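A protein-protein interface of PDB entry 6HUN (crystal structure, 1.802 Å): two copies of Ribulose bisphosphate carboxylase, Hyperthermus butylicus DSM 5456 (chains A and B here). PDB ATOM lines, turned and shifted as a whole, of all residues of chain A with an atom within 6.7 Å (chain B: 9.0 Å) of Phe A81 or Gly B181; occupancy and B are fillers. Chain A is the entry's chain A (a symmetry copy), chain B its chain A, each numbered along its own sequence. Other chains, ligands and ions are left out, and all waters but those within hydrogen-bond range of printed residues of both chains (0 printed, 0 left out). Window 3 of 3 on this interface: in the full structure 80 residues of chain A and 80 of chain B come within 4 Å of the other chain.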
ATOM      1  N   GLU A  28      -1.791  24.182  -9.850  1.00  0.00           N
ATOM      2  CA  GLU A  28      -2.472  23.626  -8.686  1.00  0.00           C
ATOM      3  C   GLU A  28      -2.260  24.454  -7.415  1.00  0.00           C
ATOM      4  O   GLU A  28      -3.001  24.274  -6.433  1.00  0.00           O
ATOM      5  CB  GLU A  28      -1.984  22.176  -8.532  1.00  0.00           C
ATOM      6  CG  GLU A  28      -1.813  21.649  -7.118  1.00  0.00           C
ATOM      7  CD  GLU A  28      -1.738  20.128  -7.034  1.00  0.00           C
ATOM      8  OE1 GLU A  28      -1.617  19.467  -8.102  1.00  0.00           O
ATOM      9  OE2 GLU A  28      -1.821  19.599  -5.892  1.00  0.00           O
ATOM     10  N   PHE A  29      -1.309  25.387  -7.417  1.00  0.00           N
ATOM     11  CA  PHE A  29      -1.023  26.189  -6.228  1.00  0.00           C
ATOM     12  C   PHE A  29      -1.534  27.614  -6.331  1.00  0.00           C
ATOM     13  O   PHE A  29      -1.260  28.417  -5.437  1.00  0.00           O
ATOM     14  CB  PHE A  29       0.491  26.200  -5.943  1.00  0.00           C
ATOM     15  CG  PHE A  29       1.032  24.850  -5.545  1.00  0.00           C
ATOM     16  CD1 PHE A  29       1.307  23.888  -6.506  1.00  0.00           C
ATOM     17  CD2 PHE A  29       1.228  24.535  -4.207  1.00  0.00           C
ATOM     18  CE1 PHE A  29       1.776  22.628  -6.161  1.00  0.00           C
ATOM     19  CE2 PHE A  29       1.708  23.286  -3.850  1.00  0.00           C
ATOM     20  CZ  PHE A  29       1.980  22.317  -4.843  1.00  0.00           C
ATOM     21  N   VAL A  68       4.894  22.435   0.384  1.00  0.00           N
ATOM     22  CA  VAL A  68       4.961  20.965   0.351  1.00  0.00           C
ATOM     23  C   VAL A  68       5.647  20.433  -0.895  1.00  0.00           C
ATOM     24  O   VAL A  68       5.632  19.221  -1.115  1.00  0.00           O
ATOM     25  CB  VAL A  68       3.560  20.331   0.457  1.00  0.00           C
ATOM     26  CG1 VAL A  68       2.951  20.701   1.768  1.00  0.00           C
ATOM     27  CG2 VAL A  68       2.714  20.802  -0.663  1.00  0.00           C
ATOM     28  N   GLY A  69       6.229  21.302  -1.727  1.00  0.00           N
ATOM     29  CA  GLY A  69       6.843  20.781  -2.938  1.00  0.00           C
ATOM     30  C   GLY A  69       5.826  20.160  -3.891  1.00  0.00           C
ATOM     31  O   GLY A  69       4.618  20.424  -3.860  1.00  0.00           O
ATOM     32  N   THR A  70       6.330  19.280  -4.737  1.00  0.00           N
ATOM     33  CA  THR A  70       5.497  18.630  -5.738  1.00  0.00           C
ATOM     34  C   THR A  70       5.650  17.118  -5.641  1.00  0.00           C
ATOM     35  O   THR A  70       6.509  16.581  -4.937  1.00  0.00           O
ATOM     36  CB  THR A  70       5.876  19.089  -7.154  1.00  0.00           C
ATOM     37  OG1 THR A  70       7.297  19.282  -7.209  1.00  0.00           O
ATOM     38  CG2 THR A  70       5.177  20.396  -7.512  1.00  0.00           C
ATOM     39  N   TRP A  71       4.822  16.423  -6.381  1.00  0.00           N
ATOM     40  CA  TRP A  71       5.090  15.005  -6.568  1.00  0.00           C
ATOM     41  C   TRP A  71       4.720  14.635  -7.990  1.00  0.00           C
ATOM     42  O   TRP A  71       3.856  15.268  -8.607  1.00  0.00           O
ATOM     43  CB  TRP A  71       4.331  14.140  -5.541  1.00  0.00           C
ATOM     44  CG  TRP A  71       2.978  13.647  -5.987  1.00  0.00           C
ATOM     45  CD1 TRP A  71       2.715  12.550  -6.748  1.00  0.00           C
ATOM     46  CD2 TRP A  71       1.708  14.248  -5.696  1.00  0.00           C
ATOM     47  NE1 TRP A  71       1.360  12.426  -6.950  1.00  0.00           N
ATOM     48  CE2 TRP A  71       0.720  13.456  -6.314  1.00  0.00           C
ATOM     49  CE3 TRP A  71       1.314  15.383  -4.979  1.00  0.00           C
ATOM     50  CZ2 TRP A  71      -0.645  13.751  -6.231  1.00  0.00           C
ATOM     51  CZ3 TRP A  71      -0.055  15.670  -4.899  1.00  0.00           C
ATOM     52  CH2 TRP A  71      -1.010  14.858  -5.522  1.00  0.00           C
ATOM     53  N   LEU A  74       3.049   8.736  -6.431  1.00  0.00           N
ATOM     54  CA  LEU A  74       3.022   8.545  -4.984  1.00  0.00           C
ATOM     55  C   LEU A  74       3.209   7.069  -4.657  1.00  0.00           C
ATOM     56  O   LEU A  74       2.355   6.245  -5.000  1.00  0.00           O
ATOM     57  CB  LEU A  74       1.712   9.045  -4.383  1.00  0.00           C
ATOM     58  CG  LEU A  74       1.683  10.512  -3.990  1.00  0.00           C
ATOM     59  CD1 LEU A  74       0.327  10.875  -3.408  1.00  0.00           C
ATOM     60  CD2 LEU A  74       2.834  10.818  -3.042  1.00  0.00           C
ATOM     61  N   LYS A  77       1.042   7.295   0.550  1.00  0.00           N
ATOM     62  CA  LYS A  77       0.177   8.471   0.578  1.00  0.00           C
ATOM     63  C   LYS A  77       0.710   9.481   1.586  1.00  0.00           C
ATOM     64  O   LYS A  77       1.037   9.096   2.714  1.00  0.00           O
ATOM     65  CB  LYS A  77      -1.254   8.087   0.942  1.00  0.00           C
ATOM     66  CG  LYS A  77      -2.021   9.150   1.711  1.00  0.00           C
ATOM     67  CD  LYS A  77      -3.531   8.983   1.608  1.00  0.00           C
ATOM     68  CE  LYS A  77      -4.255   9.460   2.868  1.00  0.00           C
ATOM     69  NZ  LYS A  77      -3.954   8.638   4.081  1.00  0.00           N
ATOM     70  N   PRO A  78       0.836  10.787   1.213  1.00  0.00           N
ATOM     71  CA  PRO A  78       1.033  11.828   2.227  1.00  0.00           C
ATOM     72  C   PRO A  78      -0.312  12.365   2.690  1.00  0.00           C
ATOM     73  O   PRO A  78      -0.953  13.158   1.988  1.00  0.00           O
ATOM     74  CB  PRO A  78       1.864  12.890   1.491  1.00  0.00           C
ATOM     75  CG  PRO A  78       1.617  12.635  -0.001  1.00  0.00           C
ATOM     76  CD  PRO A  78       0.797  11.366  -0.139  1.00  0.00           C
ATOM     77  N   SER A  79      -0.755  11.923   3.875  1.00  0.00           N
ATOM     78  CA  SER A  79      -2.066  12.318   4.378  1.00  0.00           C
ATOM     79  C   SER A  79      -2.181  13.811   4.659  1.00  0.00           C
ATOM     80  O   SER A  79      -3.292  14.284   4.903  1.00  0.00           O
ATOM     81  CB  SER A  79      -2.430  11.546   5.652  1.00  0.00           C
ATOM     82  OG  SER A  79      -1.339  11.364   6.537  1.00  0.00           O
ATOM     83  N   TRP A  80      -1.082  14.566   4.621  1.00  0.00           N
ATOM     84  CA  TRP A  80      -1.121  15.982   4.959  1.00  0.00           C
ATOM     85  C   TRP A  80      -0.745  16.895   3.794  1.00  0.00           C
ATOM     86  O   TRP A  80      -0.621  18.117   3.993  1.00  0.00           O
ATOM     87  CB  TRP A  80      -0.216  16.258   6.160  1.00  0.00           C
ATOM     88  CG  TRP A  80      -0.822  15.870   7.451  1.00  0.00           C
ATOM     89  CD1 TRP A  80      -1.009  14.602   7.915  1.00  0.00           C
ATOM     90  CD2 TRP A  80      -1.344  16.747   8.462  1.00  0.00           C
ATOM     91  NE1 TRP A  80      -1.612  14.628   9.149  1.00  0.00           N
ATOM     92  CE2 TRP A  80      -1.829  15.932   9.510  1.00  0.00           C
ATOM     93  CE3 TRP A  80      -1.460  18.137   8.580  1.00  0.00           C
ATOM     94  CZ2 TRP A  80      -2.403  16.460  10.666  1.00  0.00           C
ATOM     95  CZ3 TRP A  80      -2.042  18.661   9.739  1.00  0.00           C
ATOM     96  CH2 TRP A  80      -2.510  17.819  10.755  1.00  0.00           C
ATOM     97  N   PHE A  81      -0.608  16.355   2.580  1.00  0.00           N
ATOM     98  CA  PHE A  81      -0.155  17.166   1.451  1.00  0.00           C
ATOM     99  C   PHE A  81      -1.159  18.267   1.098  1.00  0.00           C
ATOM    100  O   PHE A  81      -0.810  19.456   1.068  1.00  0.00           O
ATOM    101  CB  PHE A  81       0.119  16.265   0.240  1.00  0.00           C
ATOM    102  CG  PHE A  81       0.542  17.019  -0.993  1.00  0.00           C
ATOM    103  CD1 PHE A  81       1.878  17.289  -1.226  1.00  0.00           C
ATOM    104  CD2 PHE A  81      -0.396  17.456  -1.915  1.00  0.00           C
ATOM    105  CE1 PHE A  81       2.281  17.976  -2.374  1.00  0.00           C
ATOM    106  CE2 PHE A  81      -0.017  18.160  -3.039  1.00  0.00           C
ATOM    107  CZ  PHE A  81       1.329  18.416  -3.280  1.00  0.00           C
ATOM    108  N   GLU A  82      -2.407  17.890   0.767  1.00  0.00           N
ATOM    109  CA  GLU A  82      -3.383  18.911   0.374  1.00  0.00           C
ATOM    110  C   GLU A  82      -3.698  19.861   1.522  1.00  0.00           C
ATOM    111  O   GLU A  82      -3.984  21.043   1.286  1.00  0.00           O
ATOM    112  CB  GLU A  82      -4.677  18.276  -0.159  1.00  0.00           C
ATOM    113  CG  GLU A  82      -4.554  17.655  -1.553  1.00  0.00           C
ATOM    114  CD  GLU A  82      -4.545  18.707  -2.667  1.00  0.00           C
ATOM    115  OE1 GLU A  82      -3.953  18.431  -3.733  1.00  0.00           O
ATOM    116  OE2 GLU A  82      -5.102  19.810  -2.479  1.00  0.00           O
ATOM    117  N   LYS A  83      -3.601  19.375   2.764  1.00  0.00           N
ATOM    118  CA  LYS A  83      -3.834  20.194   3.949  1.00  0.00           C
ATOM    119  C   LYS A  83      -2.744  21.260   4.129  1.00  0.00           C
ATOM    120  O   LYS A  83      -3.040  22.418   4.455  1.00  0.00           O
ATOM    121  CB  LYS A  83      -3.906  19.283   5.180  1.00  0.00           C
ATOM    122  CG  LYS A  83      -3.877  20.018   6.534  1.00  0.00           C
ATOM    123  CD  LYS A  83      -5.030  21.049   6.644  1.00  0.00           C
ATOM    124  CE  LYS A  83      -4.535  22.341   7.357  1.00  0.00           C
ATOM    125  NZ  LYS A  83      -5.184  23.569   6.780  1.00  0.00           N
ATOM    126  N   LEU A  84      -1.485  20.887   3.936  1.00  0.00           N
ATOM    127  CA  LEU A  84      -0.366  21.783   4.174  1.00  0.00           C
ATOM    128  C   LEU A  84      -0.057  22.698   3.001  1.00  0.00           C
ATOM    129  O   LEU A  84       0.890  23.481   3.094  1.00  0.00           O
ATOM    130  CB  LEU A  84       0.873  20.959   4.506  1.00  0.00           C
ATOM    131  CG  LEU A  84       0.826  20.217   5.828  1.00  0.00           C
ATOM    132  CD1 LEU A  84       2.070  19.353   6.024  1.00  0.00           C
ATOM    133  CD2 LEU A  84       0.675  21.241   6.966  1.00  0.00           C
ATOM    134  N   LYS A  85      -0.800  22.639   1.908  1.00  0.00           N
ATOM    135  CA  LYS A  85      -0.345  23.282   0.685  1.00  0.00           C
ATOM    136  C   LYS A  85      -0.635  24.785   0.668  1.00  0.00           C
ATOM    137  O   LYS A  85      -1.716  25.225   1.071  1.00  0.00           O
ATOM    138  CB  LYS A  85      -0.995  22.615  -0.510  1.00  0.00           C
ATOM    139  CG  LYS A  85      -0.959  23.466  -1.742  1.00  0.00           C
ATOM    140  CD  LYS A  85      -2.061  23.075  -2.672  1.00  0.00           C
ATOM    141  CE  LYS A  85      -2.055  21.588  -2.822  1.00  0.00           C
ATOM    142  NZ  LYS A  85      -2.411  21.252  -4.206  1.00  0.00           N
ATOM    143  N   ALA A  86       0.331  25.581   0.178  1.00  0.00           N
ATOM    144  CA  ALA A  86       0.165  27.038   0.140  1.00  0.00           C
ATOM    145  C   ALA A  86      -0.506  27.462  -1.167  1.00  0.00           C
ATOM    146  O   ALA A  86      -0.409  26.773  -2.182  1.00  0.00           O
ATOM    147  CB  ALA A  86       1.512  27.759   0.301  1.00  0.00           C
ATOM    148  N   PRO B 176      12.650  12.876  -0.204  1.00  0.00           N
ATOM    149  CA  PRO B 176      11.311  12.416  -0.591  1.00  0.00           C
ATOM    150  C   PRO B 176      10.519  13.462  -1.361  1.00  0.00           C
ATOM    151  O   PRO B 176      10.740  14.667  -1.262  1.00  0.00           O
ATOM    152  CB  PRO B 176      10.642  12.114   0.755  1.00  0.00           C
ATOM    153  CG  PRO B 176      11.774  11.780   1.667  1.00  0.00           C
ATOM    154  CD  PRO B 176      12.949  12.605   1.213  1.00  0.00           C
ATOM    155  N   LYS B 177       9.582  12.971  -2.152  1.00  0.00           N
ATOM    156  CA  LYS B 177       8.608  13.817  -2.783  1.00  0.00           C
ATOM    157  C   LYS B 177       7.232  13.300  -2.396  1.00  0.00           C
ATOM    158  O   LYS B 177       6.994  12.086  -2.468  1.00  0.00           O
ATOM    159  CB  LYS B 177       8.762  13.833  -4.309  1.00  0.00           C
ATOM    160  CG  LYS B 177      10.039  14.496  -4.804  1.00  0.00           C
ATOM    161  CD  LYS B 177      10.176  14.371  -6.338  1.00  0.00           C
ATOM    162  CE  LYS B 177       9.220  15.314  -7.117  1.00  0.00           C
ATOM    163  NZ  LYS B 177       9.746  16.711  -7.208  1.00  0.00           N
ATOM    164  N   PRO B 178       6.309  14.171  -1.946  1.00  0.00           N
ATOM    165  CA  PRO B 178       6.540  15.612  -1.740  1.00  0.00           C
ATOM    166  C   PRO B 178       7.414  15.859  -0.524  1.00  0.00           C
ATOM    167  O   PRO B 178       7.553  14.941   0.296  1.00  0.00           O
ATOM    168  CB  PRO B 178       5.133  16.155  -1.520  1.00  0.00           C
ATOM    169  CG  PRO B 178       4.386  14.961  -0.917  1.00  0.00           C
ATOM    170  CD  PRO B 178       4.928  13.768  -1.612  1.00  0.00           C
ATOM    171  N   LYS B 179       7.980  17.063  -0.388  1.00  0.00           N
ATOM    172  CA  LYS B 179       8.918  17.298   0.702  1.00  0.00           C
ATOM    173  C   LYS B 179       8.213  17.368   2.049  1.00  0.00           C
ATOM    174  O   LYS B 179       8.851  17.119   3.077  1.00  0.00           O
ATOM    175  CB  LYS B 179       9.742  18.571   0.453  1.00  0.00           C
ATOM    176  CG  LYS B 179       8.954  19.719  -0.194  1.00  0.00           C
ATOM    177  CD  LYS B 179       9.823  20.825  -0.777  1.00  0.00           C
ATOM    178  CE  LYS B 179       9.722  22.120   0.041  1.00  0.00           C
ATOM    179  NZ  LYS B 179      10.872  23.027  -0.291  1.00  0.00           N
ATOM    180  N   LEU B 180       6.911  17.672   2.074  1.00  0.00           N
ATOM    181  CA  LEU B 180       6.149  17.632   3.318  1.00  0.00           C
ATOM    182  C   LEU B 180       4.803  16.976   3.065  1.00  0.00           C
ATOM    183  O   LEU B 180       4.307  16.946   1.936  1.00  0.00           O
ATOM    184  CB  LEU B 180       5.934  19.030   3.931  1.00  0.00           C
ATOM    185  CG  LEU B 180       7.105  19.771   4.589  1.00  0.00           C
ATOM    186  CD1 LEU B 180       6.603  21.072   5.219  1.00  0.00           C
ATOM    187  CD2 LEU B 180       7.854  18.955   5.622  1.00  0.00           C
ATOM    188  N   GLY B 181       4.232  16.418   4.134  1.00  0.00           N
ATOM    189  CA  GLY B 181       2.896  15.833   4.057  1.00  0.00           C
ATOM    190  C   GLY B 181       2.761  14.412   4.593  1.00  0.00           C
ATOM    191  O   GLY B 181       1.651  13.880   4.673  1.00  0.00           O
ATOM    192  N   TYR B 182       3.882  13.790   4.953  1.00  0.00           N
ATOM    193  CA  TYR B 182       3.935  12.421   5.447  1.00  0.00           C
ATOM    194  C   TYR B 182       3.856  12.390   6.976  1.00  0.00           C
ATOM    195  O   TYR B 182       4.518  13.177   7.664  1.00  0.00           O
ATOM    196  CB  TYR B 182       5.238  11.748   4.976  1.00  0.00           C
ATOM    197  CG  TYR B 182       5.297  11.452   3.486  1.00  0.00           C
ATOM    198  CD1 TYR B 182       4.417  10.535   2.916  1.00  0.00           C
ATOM    199  CD2 TYR B 182       6.220  12.092   2.650  1.00  0.00           C
ATOM    200  CE1 TYR B 182       4.448  10.254   1.565  1.00  0.00           C
ATOM    201  CE2 TYR B 182       6.260  11.820   1.275  1.00  0.00           C
ATOM    202  CZ  TYR B 182       5.367  10.898   0.744  1.00  0.00           C
ATOM    203  OH  TYR B 182       5.357  10.580  -0.606  1.00  0.00           O
ATOM    204  N   THR B 183       3.062  11.465   7.509  1.00  0.00           N
ATOM    205  CA  THR B 183       3.167  11.148   8.928  1.00  0.00           C
ATOM    206  C   THR B 183       4.466  10.375   9.180  1.00  0.00           C
ATOM    207  O   THR B 183       5.133   9.936   8.237  1.00  0.00           O
ATOM    208  CB  THR B 183       1.944  10.354   9.395  1.00  0.00           C
ATOM    209  OG1 THR B 183       1.867   9.122   8.673  1.00  0.00           O
ATOM    210  CG2 THR B 183       0.676  11.161   9.175  1.00  0.00           C
ATOM    211  N   PRO B 184       4.888  10.238  10.444  1.00  0.00           N
ATOM    212  CA  PRO B 184       6.090   9.432  10.698  1.00  0.00           C
ATOM    213  C   PRO B 184       6.006   8.049  10.074  1.00  0.00           C
ATOM    214  O   PRO B 184       6.944   7.649   9.369  1.00  0.00           O
ATOM    215  CB  PRO B 184       6.156   9.394  12.222  1.00  0.00           C
ATOM    216  CG  PRO B 184       5.554  10.717  12.638  1.00  0.00           C
ATOM    217  CD  PRO B 184       4.438  10.951  11.662  1.00  0.00           C
ATOM    218  N   GLU B 186       4.256   7.032   7.501  1.00  0.00           N
ATOM    219  CA  GLU B 186       4.327   7.135   6.046  1.00  0.00           C
ATOM    220  C   GLU B 186       5.733   7.499   5.584  1.00  0.00           C
ATOM    221  O   GLU B 186       6.274   6.875   4.666  1.00  0.00           O
ATOM    222  CB  GLU B 186       3.295   8.142   5.525  1.00  0.00           C
ATOM    223  CG  GLU B 186       1.837   7.734   5.793  1.00  0.00           C
ATOM    224  CD  GLU B 186       0.848   8.913   5.768  1.00  0.00           C
ATOM    225  OE1 GLU B 186       1.279  10.076   5.528  1.00  0.00           O
ATOM    226  OE2 GLU B 186      -0.368   8.673   5.989  1.00  0.00           O
ATOM    227  N   TYR B 187       6.351   8.502   6.220  1.00  0.00           N
ATOM    228  CA  TYR B 187       7.730   8.855   5.879  1.00  0.00           C
ATOM    229  C   TYR B 187       8.690   7.666   5.991  1.00  0.00           C
ATOM    230  O   TYR B 187       9.635   7.545   5.202  1.00  0.00           O
ATOM    231  CB  TYR B 187       8.197   9.976   6.788  1.00  0.00           C
ATOM    232  CG  TYR B 187       9.306  10.822   6.226  1.00  0.00           C
ATOM    233  CD1 TYR B 187      10.559  10.841   6.831  1.00  0.00           C
ATOM    234  CD2 TYR B 187       9.098  11.625   5.109  1.00  0.00           C
ATOM    235  CE1 TYR B 187      11.578  11.652   6.346  1.00  0.00           C
ATOM    236  CE2 TYR B 187      10.121  12.451   4.629  1.00  0.00           C
ATOM    237  CZ  TYR B 187      11.360  12.432   5.251  1.00  0.00           C
ATOM    238  OH  TYR B 187      12.409  13.224   4.800  1.00  0.00           O
ATOM    239  N   VAL B 190       8.473   5.430   2.933  1.00  0.00           N
ATOM    240  CA  VAL B 190       9.087   6.084   1.773  1.00  0.00           C
ATOM    241  C   VAL B 190      10.603   5.938   1.810  1.00  0.00           C
ATOM    242  O   VAL B 190      11.246   5.695   0.775  1.00  0.00           O
ATOM    243  CB  VAL B 190       8.672   7.572   1.692  1.00  0.00           C
ATOM    244  CG1 VAL B 190       9.343   8.263   0.500  1.00  0.00           C
ATOM    245  CG2 VAL B 190       7.161   7.707   1.569  1.00  0.00           C
ATOM    246  N   ASN B 207      12.912  22.593   5.026  1.00  0.00           N
ATOM    247  CA  ASN B 207      11.913  23.180   5.911  1.00  0.00           C
ATOM    248  C   ASN B 207      11.269  22.125   6.782  1.00  0.00           C
ATOM    249  O   ASN B 207      10.283  22.393   7.466  1.00  0.00           O
ATOM    250  CB  ASN B 207      10.879  24.022   5.123  1.00  0.00           C
ATOM    251  CG  ASN B 207      10.022  23.214   4.201  1.00  0.00           C
ATOM    252  OD1 ASN B 207      10.300  22.056   3.963  1.00  0.00           O
ATOM    253  ND2 ASN B 207       8.938  23.809   3.701  1.00  0.00           N
ATOM    254  N   PHE B 208      11.832  20.920   6.796  1.00  0.00           N
ATOM    255  CA  PHE B 208      11.378  19.902   7.739  1.00  0.00           C
ATOM    256  C   PHE B 208      12.070  20.193   9.058  1.00  0.00           C
ATOM    257  O   PHE B 208      13.270  20.491   9.071  1.00  0.00           O
ATOM    258  CB  PHE B 208      11.736  18.522   7.239  1.00  0.00           C
ATOM    259  CG  PHE B 208      10.722  17.481   7.568  1.00  0.00           C
ATOM    260  CD1 PHE B 208       9.681  17.754   8.460  1.00  0.00           C
ATOM    261  CD2 PHE B 208      10.821  16.210   7.027  1.00  0.00           C
ATOM    262  CE1 PHE B 208       8.739  16.799   8.804  1.00  0.00           C
ATOM    263  CE2 PHE B 208       9.886  15.245   7.363  1.00  0.00           C
ATOM    264  CZ  PHE B 208       8.836  15.545   8.266  1.00  0.00           C
ATOM    265  N   GLN B 211       7.429  19.977  13.026  1.00  0.00           N
ATOM    266  CA  GLN B 211       6.021  20.349  12.970  1.00  0.00           C
ATOM    267  C   GLN B 211       5.131  19.282  13.606  1.00  0.00           C
ATOM    268  O   GLN B 211       5.505  18.108  13.677  1.00  0.00           O
ATOM    269  CB  GLN B 211       5.603  20.566  11.521  1.00  0.00           C
ATOM    270  CG  GLN B 211       6.283  21.782  10.867  1.00  0.00           C
ATOM    271  CD  GLN B 211       7.561  21.439  10.096  1.00  0.00           C
ATOM    272  OE1 GLN B 211       8.307  20.540  10.463  1.00  0.00           O
ATOM    273  NE2 GLN B 211       7.800  22.163   9.013  1.00  0.00           N
ATOM    274  N   PHE B 213       2.532  17.620  12.585  1.00  0.00           N
ATOM    275  CA  PHE B 213       2.044  16.467  11.837  1.00  0.00           C
ATOM    276  C   PHE B 213       3.087  15.361  11.746  1.00  0.00           C
ATOM    277  O   PHE B 213       2.736  14.238  11.374  1.00  0.00           O
ATOM    278  CB  PHE B 213       1.583  16.880  10.435  1.00  0.00           C
ATOM    279  CG  PHE B 213       2.707  17.253   9.518  1.00  0.00           C
ATOM    280  CD1 PHE B 213       3.305  16.300   8.702  1.00  0.00           C
ATOM    281  CD2 PHE B 213       3.175  18.562   9.473  1.00  0.00           C
ATOM    282  CE1 PHE B 213       4.350  16.635   7.862  1.00  0.00           C
ATOM    283  CE2 PHE B 213       4.232  18.913   8.622  1.00  0.00           C
ATOM    284  CZ  PHE B 213       4.821  17.933   7.833  1.00  0.00           C
ATOM    285  N   CYS B 214       4.336  15.650  12.112  1.00  0.00           N
ATOM    286  CA  CYS B 214       5.471  14.739  11.973  1.00  0.00           C
ATOM    287  C   CYS B 214       6.627  15.219  12.843  1.00  0.00           C
ATOM    288  O   CYS B 214       7.608  15.798  12.351  1.00  0.00           O
ATOM    289  CB  CYS B 214       5.941  14.637  10.516  1.00  0.00           C
ATOM    290  SG  CYS B 214       6.969  13.150  10.201  1.00  0.00           S
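OE1 of Glu B186 lies close to O of Lys A77. O of Gly B181 lies within hydrogen-bond range of N of Ser A79 (3.2 Å). OG of Ser A79 sits at hydrogen-bond distance from OE2 of Glu B186 (2.9 Å). O of Gly B181 is in hydrogen-bond range of N of Trp A80. The backbone carbonyl oxygen of Val A68 is in hydrogen-bond range of the backbone NH of Lys B179 (3.3 Å).
CG of Lys B179 touches N of Gly A69, at 3.5 Å. Pro B178 touches Thr A70 (CA to O, 3.3 Å). Pro B178 touches Leu A74 (CD to CD2, 3.9 Å). CD2 of Leu A74 touches OH of Tyr B182, 3.5 Å away. Tyr B182 touches Lys A77 (CD1 to O, 3.7 Å). CG of Pro A78 touches CG of Pro B178, 3.7 Å away. Pro A78 touches Gly B181. Tyr B182 touches Pro A78. CA of Pro A78 touches OE1 of Glu B186, 3.7 Å away. Ser A79 touches Thr B183 (OG to CG2, 3.3 Å).
Printed residues of chain B within 4 Å of Thr A70: Lys B177 (3.6 Å) and Pro B178 (3.3 Å). Of the printed residues of chain B, Pro A78 touches Pro B178 (3.7 Å), Gly B181 (3.2 Å), Tyr B182 (3.7 Å) and Glu B186 (3.7 Å). Of chain B, only Gly B181, Thr B183 and Glu B186 come within 4 Å of Ser A79. Printed residues of chain B within 4 Å of Trp A80: Gly B181 and Phe B213. Of the printed residues of chain B, Phe A81 touches Pro B178 (3.4 Å) and Gly B181 (3.8 Å). Of chain A, only Pro A78, Ser A79, Trp A80 and Phe A81 come within 4 Å of Gly B181. Printed residues of chain A within 4 Å of Tyr B182: Leu A74 (3.5 Å), Lys A77 (3.7 Å) and Pro A78 (3.7 Å). Of the printed residues of chain A, Glu B186 touches Lys A77 (3.0 Å), Pro A78 (3.7 Å) and Ser A79 (2.9 Å). The nearest printed residue of chain B that does not touch Phe A81 is Leu B180 (4.002 Å). The nearest printed residue of chain B that does not touch Lys A77 is Gly B181 (5.2 Å).
Printed residues of chain A that touch a printed residue of chain B: Val A68, Gly A69, Thr A70, Trp A71, Leu A74, Lys A77, Pro A78, Ser A79, Trp A80, Phe A81 and Leu A84. Of the 17 printed residues of chain B, 9 touch a printed residue of chain A. Printed residues of chain B that touch a printed residue of chain A: Lys B177, Pro B178, Lys B179, Leu B180, Gly B181, Tyr B182, Thr B183, Glu B186 and Phe B213. Hydrophobic or aromatic side chains of chain B within 4 Å of the printed part of chain A: Pro B178, Tyr B182 and Phe B213. Among the printed residues, no Asp or Glu carboxylate lies within 4 Å of a Lys or Arg side-chain nitrogen of the other chain.
O of Lys B177 sits at hydrogen-bond distance from OH of Tyr B182 (2.9 Å). OE1 of Glu B186 sits at hydrogen-bond distance from N of Thr B183, at 3.0 Å. SG of Cys B214 sits close to O of Tyr B182.
No position is printed for both chains. Of the 23 pairs that touch across the chains among the printed residues, none has its exchanged pair printed and touching as well.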
